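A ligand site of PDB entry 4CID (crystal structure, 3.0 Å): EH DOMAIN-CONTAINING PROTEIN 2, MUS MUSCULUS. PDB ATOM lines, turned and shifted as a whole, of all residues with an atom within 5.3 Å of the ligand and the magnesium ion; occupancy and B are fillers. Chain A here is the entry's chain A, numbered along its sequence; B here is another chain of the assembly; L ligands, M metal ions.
Within 4 Å of the magnesium ion: Thr 79 and Thr 101.
The magnesium ion is bound by O3 of the ligand (1.9 Å), OG1 of Thr 79 (2.1 Å), O5 of the ligand (2.2 Å) and OG1 of Thr 101 (2.5 Å).
OG of Ser 75 is in hydrogen-bond range of O of Pro 97 (2.6 Å). The side-chain carboxylate (OD2) of Asp 160 sits close to the side-chain hydroxyl (OG1) of Thr 79 (2.8 Å). The side-chain amino group of Lys 78 is in hydrogen-bond range of the backbone carbonyl oxygen of Thr 161. The side-chain amino group of Lys 227 lies within hydrogen-bond range of the backbone carbonyl oxygen of Ser 75. The backbone carbonyl oxygen (O) of Gly 163 lies close to the side-chain hydroxyl (OH) of Tyr 74, at 3.3 Å. The side-chain amide oxygen of Asn 226 sits at hydrogen-bond distance from the backbone NH of Phe 264, 3.1 Å away. The side-chain amide nitrogen (ND2) of Asn 226 lies within hydrogen-bond range of the backbone carbonyl oxygen (O) of Thr 76 (3.0 Å). OG1 of Thr 76 sits at hydrogen-bond distance from O of Gln 73 (2.5 Å).
O1 of the ligand is in salt-bridge range of NZ of Lys 78. The backbone NH of Lys 78 lies within hydrogen-bond range of an oxygen (O4) of the ligand (3.1 Å). O4 of the ligand lies within hydrogen-bond range of N of Gly 77 (3.0 Å). O7 of the ligand is in hydrogen-bond range of OG of Ser 80, 2.5 Å away. An oxygen (O6) of the ligand sits at hydrogen-bond distance from the backbone NH (N) of Gly 96, 3.3 Å away. The backbone NH (N) of Ser 75 sits at hydrogen-bond distance from an oxygen (O1) of the ligand (3.2 Å). An oxygen (O10) of the ligand lies within hydrogen-bond range of the side-chain amino group (NZ) of Lys 227. O5 of the ligand lies close to N of Thr 79, 3.1 Å away. The backbone NH (N) of Ser 80 lies within hydrogen-bond range of an oxygen (O7) of the ligand (2.9 Å). An oxygen (O2) of the ligand is in hydrogen-bond range of the backbone NH of Thr 100, 3.3 Å away. OD1 of Asn 226 lies within hydrogen-bond range of N4 of the ligand. An oxygen (O4) of the ligand is in hydrogen-bond range of the backbone NH (N) of Thr 76, at 3.2 Å.
Merely in contact with the ligand: Gln 73, Tyr 74, Val 95, Pro 97, Pro 99, Gly 163, Met 230, Ser 263, Phe 264 and Trp 265. Of the 30 residues printed, 21 come within 4 Å of the ligand.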
ATOM      1  N   GLY A  72       6.070  27.499  25.053  1.00  0.00           N
ATOM      2  CA  GLY A  72       6.946  28.648  25.196  1.00  0.00           C
ATOM      3  C   GLY A  72       6.828  29.620  24.040  1.00  0.00           C
ATOM      4  O   GLY A  72       6.071  29.383  23.091  1.00  0.00           O
ATOM      5  N   GLN A  73       7.574  30.708  24.124  1.00  0.00           N
ATOM      6  CA  GLN A  73       7.518  31.753  23.121  1.00  0.00           C
ATOM      7  C   GLN A  73       8.323  31.346  21.890  1.00  0.00           C
ATOM      8  O   GLN A  73       8.857  30.243  21.839  1.00  0.00           O
ATOM      9  CB  GLN A  73       8.009  33.083  23.688  1.00  0.00           C
ATOM     10  CG  GLN A  73       7.269  33.504  24.945  1.00  0.00           C
ATOM     11  CD  GLN A  73       7.230  35.001  25.167  1.00  0.00           C
ATOM     12  OE1 GLN A  73       6.260  35.526  25.707  1.00  0.00           O
ATOM     13  NE2 GLN A  73       8.276  35.696  24.747  1.00  0.00           N
ATOM     14  N   TYR A  74       8.391  32.230  20.903  1.00  0.00           N
ATOM     15  CA  TYR A  74       9.101  31.913  19.680  1.00  0.00           C
ATOM     16  C   TYR A  74      10.600  31.764  19.932  1.00  0.00           C
ATOM     17  O   TYR A  74      11.186  32.507  20.718  1.00  0.00           O
ATOM     18  CB  TYR A  74       8.836  32.976  18.603  1.00  0.00           C
ATOM     19  CG  TYR A  74       7.443  32.883  18.031  1.00  0.00           C
ATOM     20  CD1 TYR A  74       7.035  31.764  17.318  1.00  0.00           C
ATOM     21  CD2 TYR A  74       6.522  33.916  18.221  1.00  0.00           C
ATOM     22  CE1 TYR A  74       5.759  31.679  16.783  1.00  0.00           C
ATOM     23  CE2 TYR A  74       5.237  33.834  17.687  1.00  0.00           C
ATOM     24  CZ  TYR A  74       4.862  32.715  16.977  1.00  0.00           C
ATOM     25  OH  TYR A  74       3.594  32.618  16.453  1.00  0.00           O
ATOM     26  N   SER A  75      11.182  30.770  19.262  1.00  0.00           N
ATOM     27  CA  SER A  75      12.621  30.531  19.280  1.00  0.00           C
ATOM     28  C   SER A  75      13.166  30.275  20.682  1.00  0.00           C
ATOM     29  O   SER A  75      14.328  30.556  20.959  1.00  0.00           O
ATOM     30  CB  SER A  75      13.368  31.712  18.633  1.00  0.00           C
ATOM     31  OG  SER A  75      12.765  32.088  17.402  1.00  0.00           O
ATOM     32  N   THR A  76      12.334  29.724  21.566  1.00  0.00           N
ATOM     33  CA  THR A  76      12.782  29.406  22.913  1.00  0.00           C
ATOM     34  C   THR A  76      13.582  28.107  22.905  1.00  0.00           C
ATOM     35  O   THR A  76      14.432  27.893  23.768  1.00  0.00           O
ATOM     36  CB  THR A  76      11.605  29.269  23.886  1.00  0.00           C
ATOM     37  OG1 THR A  76      10.587  30.218  23.581  1.00  0.00           O
ATOM     38  CG2 THR A  76      12.078  29.516  25.291  1.00  0.00           C
ATOM     39  N   GLY A  77      13.304  27.248  21.938  1.00  0.00           N
ATOM     40  CA  GLY A  77      14.006  25.976  21.781  1.00  0.00           C
ATOM     41  C   GLY A  77      13.168  24.742  22.042  1.00  0.00           C
ATOM     42  O   GLY A  77      13.695  23.704  22.415  1.00  0.00           O
ATOM     43  N   LYS A  78      11.857  24.837  21.810  1.00  0.00           N
ATOM     44  CA  LYS A  78      10.945  23.733  22.100  1.00  0.00           C
ATOM     45  C   LYS A  78      11.239  22.531  21.216  1.00  0.00           C
ATOM     46  O   LYS A  78      11.443  21.404  21.696  1.00  0.00           O
ATOM     47  CB  LYS A  78       9.500  24.179  21.862  1.00  0.00           C
ATOM     48  CG  LYS A  78       9.050  25.355  22.709  1.00  0.00           C
ATOM     49  CD  LYS A  78       7.739  25.939  22.211  1.00  0.00           C
ATOM     50  CE  LYS A  78       7.936  26.779  20.967  1.00  0.00           C
ATOM     51  NZ  LYS A  78       6.825  26.560  20.005  1.00  0.00           N
ATOM     52  N   THR A  79      11.262  22.761  19.908  1.00  0.00           N
ATOM     53  CA  THR A  79      11.501  21.695  18.955  1.00  0.00           C
ATOM     54  C   THR A  79      12.886  21.098  19.194  1.00  0.00           C
ATOM     55  O   THR A  79      13.047  19.881  19.191  1.00  0.00           O
ATOM     56  CB  THR A  79      11.366  22.214  17.500  1.00  0.00           C
ATOM     57  OG1 THR A  79      10.146  22.968  17.373  1.00  0.00           O
ATOM     58  CG2 THR A  79      11.349  21.062  16.517  1.00  0.00           C
ATOM     59  N   SER A  80      13.865  21.971  19.443  1.00  0.00           N
ATOM     60  CA  SER A  80      15.227  21.529  19.770  1.00  0.00           C
ATOM     61  C   SER A  80      15.262  20.639  21.025  1.00  0.00           C
ATOM     62  O   SER A  80      15.929  19.622  21.050  1.00  0.00           O
ATOM     63  CB  SER A  80      16.137  22.742  19.970  1.00  0.00           C
ATOM     64  OG  SER A  80      16.269  23.508  18.779  1.00  0.00           O
ATOM     65  N   PHE A  81      14.529  21.056  22.055  1.00  0.00           N
ATOM     66  CA  PHE A  81      14.425  20.328  23.328  1.00  0.00           C
ATOM     67  C   PHE A  81      13.928  18.899  23.124  1.00  0.00           C
ATOM     68  O   PHE A  81      14.536  17.933  23.626  1.00  0.00           O
ATOM     69  CB  PHE A  81      13.477  21.095  24.255  1.00  0.00           C
ATOM     70  CG  PHE A  81      13.220  20.432  25.571  1.00  0.00           C
ATOM     71  CD1 PHE A  81      14.123  20.559  26.617  1.00  0.00           C
ATOM     72  CD2 PHE A  81      12.073  19.700  25.780  1.00  0.00           C
ATOM     73  CE1 PHE A  81      13.894  19.952  27.829  1.00  0.00           C
ATOM     74  CE2 PHE A  81      11.824  19.092  27.005  1.00  0.00           C
ATOM     75  CZ  PHE A  81      12.732  19.213  28.031  1.00  0.00           C
ATOM     76  N   ARG A  94      10.927  21.218  12.102  1.00  0.00           N
ATOM     77  CA  ARG A  94      12.324  21.510  11.826  1.00  0.00           C
ATOM     78  C   ARG A  94      12.770  22.705  12.666  1.00  0.00           C
ATOM     79  O   ARG A  94      11.952  23.543  13.044  1.00  0.00           O
ATOM     80  CB  ARG A  94      12.534  21.812  10.349  1.00  0.00           C
ATOM     81  CG  ARG A  94      12.213  20.632   9.430  1.00  0.00           C
ATOM     82  CD  ARG A  94      13.061  20.656   8.158  1.00  0.00           C
ATOM     83  NE  ARG A  94      14.470  20.382   8.433  1.00  0.00           N
ATOM     84  CZ  ARG A  94      15.408  20.225   7.505  1.00  0.00           C
ATOM     85  NH1 ARG A  94      15.114  20.304   6.218  1.00  0.00           N
ATOM     86  NH2 ARG A  94      16.661  19.983   7.879  1.00  0.00           N
ATOM     87  N   VAL A  95      14.073  22.770  12.931  1.00  0.00           N
ATOM     88  CA  VAL A  95      14.664  23.858  13.714  1.00  0.00           C
ATOM     89  C   VAL A  95      14.928  25.091  12.829  1.00  0.00           C
ATOM     90  O   VAL A  95      15.304  24.950  11.661  1.00  0.00           O
ATOM     91  CB  VAL A  95      15.956  23.390  14.438  1.00  0.00           C
ATOM     92  CG1 VAL A  95      17.105  23.156  13.456  1.00  0.00           C
ATOM     93  CG2 VAL A  95      16.370  24.384  15.515  1.00  0.00           C
ATOM     94  N   GLY A  96      14.723  26.283  13.389  1.00  0.00           N
ATOM     95  CA  GLY A  96      14.983  27.526  12.657  1.00  0.00           C
ATOM     96  C   GLY A  96      14.897  28.754  13.559  1.00  0.00           C
ATOM     97  O   GLY A  96      14.164  28.749  14.539  1.00  0.00           O
ATOM     98  N   PRO A  97      15.659  29.827  13.220  1.00  0.00           N
ATOM     99  CA  PRO A  97      15.688  31.042  14.049  1.00  0.00           C
ATOM    100  C   PRO A  97      14.404  31.871  14.018  1.00  0.00           C
ATOM    101  O   PRO A  97      13.950  32.360  15.055  1.00  0.00           O
ATOM    102  CB  PRO A  97      16.860  31.842  13.467  1.00  0.00           C
ATOM    103  CG  PRO A  97      16.964  31.384  12.055  1.00  0.00           C
ATOM    104  CD  PRO A  97      16.476  29.970  12.001  1.00  0.00           C
ATOM    105  N   GLU A  98      13.812  32.012  12.824  1.00  0.00           N
ATOM    106  CA  GLU A  98      12.559  32.734  12.636  1.00  0.00           C
ATOM    107  C   GLU A  98      11.408  31.772  12.987  1.00  0.00           C
ATOM    108  O   GLU A  98      11.627  30.559  13.002  1.00  0.00           O
ATOM    109  CB  GLU A  98      12.459  33.230  11.186  1.00  0.00           C
ATOM    110  CG  GLU A  98      11.742  34.569  10.998  1.00  0.00           C
ATOM    111  CD  GLU A  98      12.215  35.333   9.770  1.00  0.00           C
ATOM    112  OE1 GLU A  98      13.429  35.530   9.604  1.00  0.00           O
ATOM    113  OE2 GLU A  98      11.350  35.736   8.958  1.00  0.00           O
ATOM    114  N   PRO A  99      10.209  32.302  13.295  1.00  0.00           N
ATOM    115  CA  PRO A  99       9.060  31.424  13.584  1.00  0.00           C
ATOM    116  C   PRO A  99       8.816  30.329  12.526  1.00  0.00           C
ATOM    117  O   PRO A  99       8.321  30.619  11.439  1.00  0.00           O
ATOM    118  CB  PRO A  99       7.883  32.406  13.646  1.00  0.00           C
ATOM    119  CG  PRO A  99       8.497  33.658  14.157  1.00  0.00           C
ATOM    120  CD  PRO A  99       9.889  33.713  13.604  1.00  0.00           C
ATOM    121  N   THR A 100       9.181  29.084  12.866  1.00  0.00           N
ATOM    122  CA  THR A 100       9.104  27.953  11.933  1.00  0.00           C
ATOM    123  C   THR A 100       7.818  27.149  12.127  1.00  0.00           C
ATOM    124  O   THR A 100       6.988  27.044  11.218  1.00  0.00           O
ATOM    125  CB  THR A 100      10.331  27.016  12.082  1.00  0.00           C
ATOM    126  OG1 THR A 100      11.531  27.791  12.186  1.00  0.00           O
ATOM    127  CG2 THR A 100      10.442  26.078  10.882  1.00  0.00           C
ATOM    128  N   THR A 101       7.655  26.579  13.321  1.00  0.00           N
ATOM    129  CA  THR A 101       6.503  25.732  13.648  1.00  0.00           C
ATOM    130  C   THR A 101       5.228  26.568  13.665  1.00  0.00           C
ATOM    131  O   THR A 101       5.199  27.654  14.234  1.00  0.00           O
ATOM    132  CB  THR A 101       6.673  25.032  15.016  1.00  0.00           C
ATOM    133  OG1 THR A 101       7.960  24.384  15.096  1.00  0.00           O
ATOM    134  CG2 THR A 101       5.583  23.993  15.252  1.00  0.00           C
ATOM    135  N   ASP A 160       4.755  18.861  20.560  1.00  0.00           N
ATOM    136  CA  ASP A 160       5.350  20.153  20.197  1.00  0.00           C
ATOM    137  C   ASP A 160       4.200  21.087  19.849  1.00  0.00           C
ATOM    138  O   ASP A 160       3.324  20.739  19.051  1.00  0.00           O
ATOM    139  CB  ASP A 160       6.326  19.997  19.014  1.00  0.00           C
ATOM    140  CG  ASP A 160       7.275  21.201  18.858  1.00  0.00           C
ATOM    141  OD1 ASP A 160       7.004  22.278  19.425  1.00  0.00           O
ATOM    142  OD2 ASP A 160       8.296  21.058  18.157  1.00  0.00           O
ATOM    143  N   THR A 161       4.206  22.276  20.449  1.00  0.00           N
ATOM    144  CA  THR A 161       3.162  23.263  20.237  1.00  0.00           C
ATOM    145  C   THR A 161       3.697  24.418  19.400  1.00  0.00           C
ATOM    146  O   THR A 161       4.919  24.525  19.234  1.00  0.00           O
ATOM    147  CB  THR A 161       2.636  23.807  21.580  1.00  0.00           C
ATOM    148  OG1 THR A 161       3.682  24.485  22.282  1.00  0.00           O
ATOM    149  CG2 THR A 161       2.101  22.668  22.446  1.00  0.00           C
ATOM    150  N   PRO A 162       2.802  25.275  18.856  1.00  0.00           N
ATOM    151  CA  PRO A 162       3.262  26.503  18.199  1.00  0.00           C
ATOM    152  C   PRO A 162       3.799  27.542  19.184  1.00  0.00           C
ATOM    153  O   PRO A 162       3.405  27.551  20.361  1.00  0.00           O
ATOM    154  CB  PRO A 162       1.988  27.035  17.504  1.00  0.00           C
ATOM    155  CG  PRO A 162       1.021  25.903  17.501  1.00  0.00           C
ATOM    156  CD  PRO A 162       1.351  25.068  18.700  1.00  0.00           C
ATOM    157  N   GLY A 163       4.695  28.400  18.712  1.00  0.00           N
ATOM    158  CA  GLY A 163       5.316  29.403  19.561  1.00  0.00           C
ATOM    159  C   GLY A 163       4.316  30.425  20.045  1.00  0.00           C
ATOM    160  O   GLY A 163       3.472  30.893  19.272  1.00  0.00           O
ATOM    161  N   ASN A 226      16.208  27.941  29.355  1.00  0.00           N
ATOM    162  CA  ASN A 226      17.042  27.437  28.285  1.00  0.00           C
ATOM    163  C   ASN A 226      18.129  28.423  27.882  1.00  0.00           C
ATOM    164  O   ASN A 226      18.037  29.626  28.161  1.00  0.00           O
ATOM    165  CB  ASN A 226      16.174  27.110  27.062  1.00  0.00           C
ATOM    166  CG  ASN A 226      16.786  26.060  26.166  1.00  0.00           C
ATOM    167  OD1 ASN A 226      17.743  25.390  26.561  1.00  0.00           O
ATOM    168  ND2 ASN A 226      16.249  25.900  24.968  1.00  0.00           N
ATOM    169  N   LYS A 227      19.158  27.897  27.228  1.00  0.00           N
ATOM    170  CA  LYS A 227      20.259  28.675  26.673  1.00  0.00           C
ATOM    171  C   LYS A 227      21.105  29.367  27.732  1.00  0.00           C
ATOM    172  O   LYS A 227      21.811  30.315  27.421  1.00  0.00           O
ATOM    173  CB  LYS A 227      19.749  29.722  25.668  1.00  0.00           C
ATOM    174  CG  LYS A 227      18.688  29.215  24.711  1.00  0.00           C
ATOM    175  CD  LYS A 227      18.454  30.149  23.532  1.00  0.00           C
ATOM    176  CE  LYS A 227      17.213  29.722  22.755  1.00  0.00           C
ATOM    177  NZ  LYS A 227      16.911  30.610  21.605  1.00  0.00           N
ATOM    178  N   ASP A 229      23.839  28.786  28.952  1.00  0.00           N
ATOM    179  CA  ASP A 229      25.261  28.853  28.566  1.00  0.00           C
ATOM    180  C   ASP A 229      25.584  29.992  27.588  1.00  0.00           C
ATOM    181  O   ASP A 229      26.739  30.131  27.185  1.00  0.00           O
ATOM    182  CB  ASP A 229      25.699  27.538  27.923  1.00  0.00           C
ATOM    183  CG  ASP A 229      25.119  27.344  26.533  1.00  0.00           C
ATOM    184  OD1 ASP A 229      23.982  27.805  26.282  1.00  0.00           O
ATOM    185  OD2 ASP A 229      25.798  26.722  25.683  1.00  0.00           O
ATOM    186  N   MET A 230      24.569  30.761  27.202  1.00  0.00           N
ATOM    187  CA  MET A 230      24.740  31.863  26.249  1.00  0.00           C
ATOM    188  C   MET A 230      25.030  33.168  26.921  1.00  0.00           C
ATOM    189  O   MET A 230      25.772  33.993  26.382  1.00  0.00           O
ATOM    190  CB  MET A 230      23.440  32.008  25.464  1.00  0.00           C
ATOM    191  CG  MET A 230      23.631  32.607  24.087  1.00  0.00           C
ATOM    192  SD  MET A 230      22.260  31.812  22.910  1.00  0.00           S
ATOM    193  CE  MET A 230      23.048  32.353  21.184  1.00  0.00           C
ATOM    194  N   SER A 263      20.998  24.410  28.959  1.00  0.00           N
ATOM    195  CA  SER A 263      20.941  24.545  27.515  1.00  0.00           C
ATOM    196  C   SER A 263      20.714  23.140  26.945  1.00  0.00           C
ATOM    197  O   SER A 263      21.634  22.343  26.850  1.00  0.00           O
ATOM    198  CB  SER A 263      22.220  25.216  26.969  1.00  0.00           C
ATOM    199  OG  SER A 263      23.185  24.281  26.533  1.00  0.00           O
ATOM    200  N   PHE A 264      19.463  22.855  26.595  1.00  0.00           N
ATOM    201  CA  PHE A 264      19.038  21.520  26.179  1.00  0.00           C
ATOM    202  C   PHE A 264      19.292  21.360  24.689  1.00  0.00           C
ATOM    203  O   PHE A 264      18.441  21.620  23.841  1.00  0.00           O
ATOM    204  CB  PHE A 264      17.591  21.296  26.600  1.00  0.00           C
ATOM    205  CG  PHE A 264      17.402  21.346  28.091  1.00  0.00           C
ATOM    206  CD1 PHE A 264      17.352  22.558  28.761  1.00  0.00           C
ATOM    207  CD2 PHE A 264      17.322  20.169  28.830  1.00  0.00           C
ATOM    208  CE1 PHE A 264      17.200  22.606  30.142  1.00  0.00           C
ATOM    209  CE2 PHE A 264      17.179  20.213  30.209  1.00  0.00           C
ATOM    210  CZ  PHE A 264      17.106  21.430  30.863  1.00  0.00           C
ATOM    211  N   TRP A 265      20.500  20.897  24.412  1.00  0.00           N
ATOM    212  CA  TRP A 265      21.282  21.332  23.286  1.00  0.00           C
ATOM    213  C   TRP A 265      22.477  20.379  23.186  1.00  0.00           C
ATOM    214  O   TRP A 265      23.279  20.263  24.129  1.00  0.00           O
ATOM    215  CB  TRP A 265      21.782  22.737  23.647  1.00  0.00           C
ATOM    216  CG  TRP A 265      22.345  23.586  22.575  1.00  0.00           C
ATOM    217  CD1 TRP A 265      23.489  24.318  22.634  1.00  0.00           C
ATOM    218  CD2 TRP A 265      21.765  23.846  21.292  1.00  0.00           C
ATOM    219  NE1 TRP A 265      23.669  25.005  21.464  1.00  0.00           N
ATOM    220  CE2 TRP A 265      22.629  24.729  20.618  1.00  0.00           C
ATOM    221  CE3 TRP A 265      20.612  23.401  20.644  1.00  0.00           C
ATOM    222  CZ2 TRP A 265      22.374  25.184  19.328  1.00  0.00           C
ATOM    223  CZ3 TRP A 265      20.359  23.857  19.364  1.00  0.00           C
ATOM    224  CH2 TRP A 265      21.239  24.740  18.717  1.00  0.00           C
ATOM    225  N   ARG B 544      30.401  26.171  17.368  1.00  0.00           N
ATOM    226  CA  ARG B 544      29.138  26.903  17.376  1.00  0.00           C
ATOM    227  C   ARG B 544      29.043  27.837  16.179  1.00  0.00           C
ATOM    228  O   ARG B 544      30.061  28.282  15.651  1.00  0.00           O
ATOM    229  CB  ARG B 544      29.006  27.733  18.645  1.00  0.00           C
ATOM    230  CG  ARG B 544      28.851  26.929  19.927  1.00  0.00           C
ATOM    231  CD  ARG B 544      28.830  27.846  21.132  1.00  0.00           C
ATOM    232  NE  ARG B 544      27.626  28.676  21.198  1.00  0.00           N
ATOM    233  CZ  ARG B 544      26.469  28.309  21.753  1.00  0.00           C
ATOM    234  NH1 ARG B 544      26.320  27.110  22.313  1.00  0.00           N
ATOM    235  NH2 ARG B 544      25.444  29.149  21.761  1.00  0.00           N
HETATM  236  P1  LIG L   1       9.123  28.043  17.344  1.00  0.00           P
HETATM  237  O1  LIG L   1       8.732  28.733  18.631  1.00  0.00           O
HETATM  238  O2  LIG L   1       8.925  28.915  16.134  1.00  0.00           O
HETATM  239  O3  LIG L   1       8.638  26.621  17.198  1.00  0.00           O
HETATM  240  P2  LIG L   1      11.475  26.790  18.724  1.00  0.00           P
HETATM  241  O4  LIG L   1      10.950  27.287  20.052  1.00  0.00           O
HETATM  242  O5  LIG L   1      11.215  25.358  18.288  1.00  0.00           O
HETATM  243  N1  LIG L   1      10.853  27.840  17.474  1.00  0.00           N
HETATM  244  P3  LIG L   1      14.035  26.131  17.913  1.00  0.00           P
HETATM  245  O6  LIG L   1      13.619  26.313  16.484  1.00  0.00           O
HETATM  246  O7  LIG L   1      14.133  24.733  18.469  1.00  0.00           O
HETATM  247  O8  LIG L   1      13.051  27.004  18.823  1.00  0.00           O
HETATM  248  O9  LIG L   1      15.402  26.947  18.153  1.00  0.00           O
HETATM  249  C1  LIG L   1      15.384  28.366  18.072  1.00  0.00           C
HETATM  250  C2  LIG L   1      16.753  28.889  17.650  1.00  0.00           C
HETATM  251  O10 LIG L   1      17.592  28.952  18.799  1.00  0.00           O
HETATM  252  C3  LIG L   1      17.455  28.007  16.622  1.00  0.00           C
HETATM  253  O11 LIG L   1      18.097  28.810  15.622  1.00  0.00           O
HETATM  254  C4  LIG L   1      18.458  27.216  17.424  1.00  0.00           C
HETATM  255  O12 LIG L   1      19.682  27.018  16.700  1.00  0.00           O
HETATM  256  C5  LIG L   1      18.693  28.049  18.670  1.00  0.00           C
HETATM  257  N2  LIG L   1      18.767  27.239  19.908  1.00  0.00           N
HETATM  258  C6  LIG L   1      17.928  26.240  20.263  1.00  0.00           C
HETATM  259  N3  LIG L   1      18.284  25.719  21.459  1.00  0.00           N
HETATM  260  C7  LIG L   1      19.353  26.398  21.878  1.00  0.00           C
HETATM  261  C8  LIG L   1      20.220  26.351  23.067  1.00  0.00           C
HETATM  262  N4  LIG L   1      19.936  25.431  24.020  1.00  0.00           N
HETATM  263  N5  LIG L   1      21.243  27.231  23.162  1.00  0.00           N
HETATM  264  C9  LIG L   1      21.486  28.141  22.188  1.00  0.00           C
HETATM  265  N6  LIG L   1      20.733  28.227  21.075  1.00  0.00           N
HETATM  266  C10 LIG L   1      19.672  27.403  20.867  1.00  0.00           C
HETATM  267 MG    MG M   1       9.463  24.947  17.036  1.00  0.00          MG
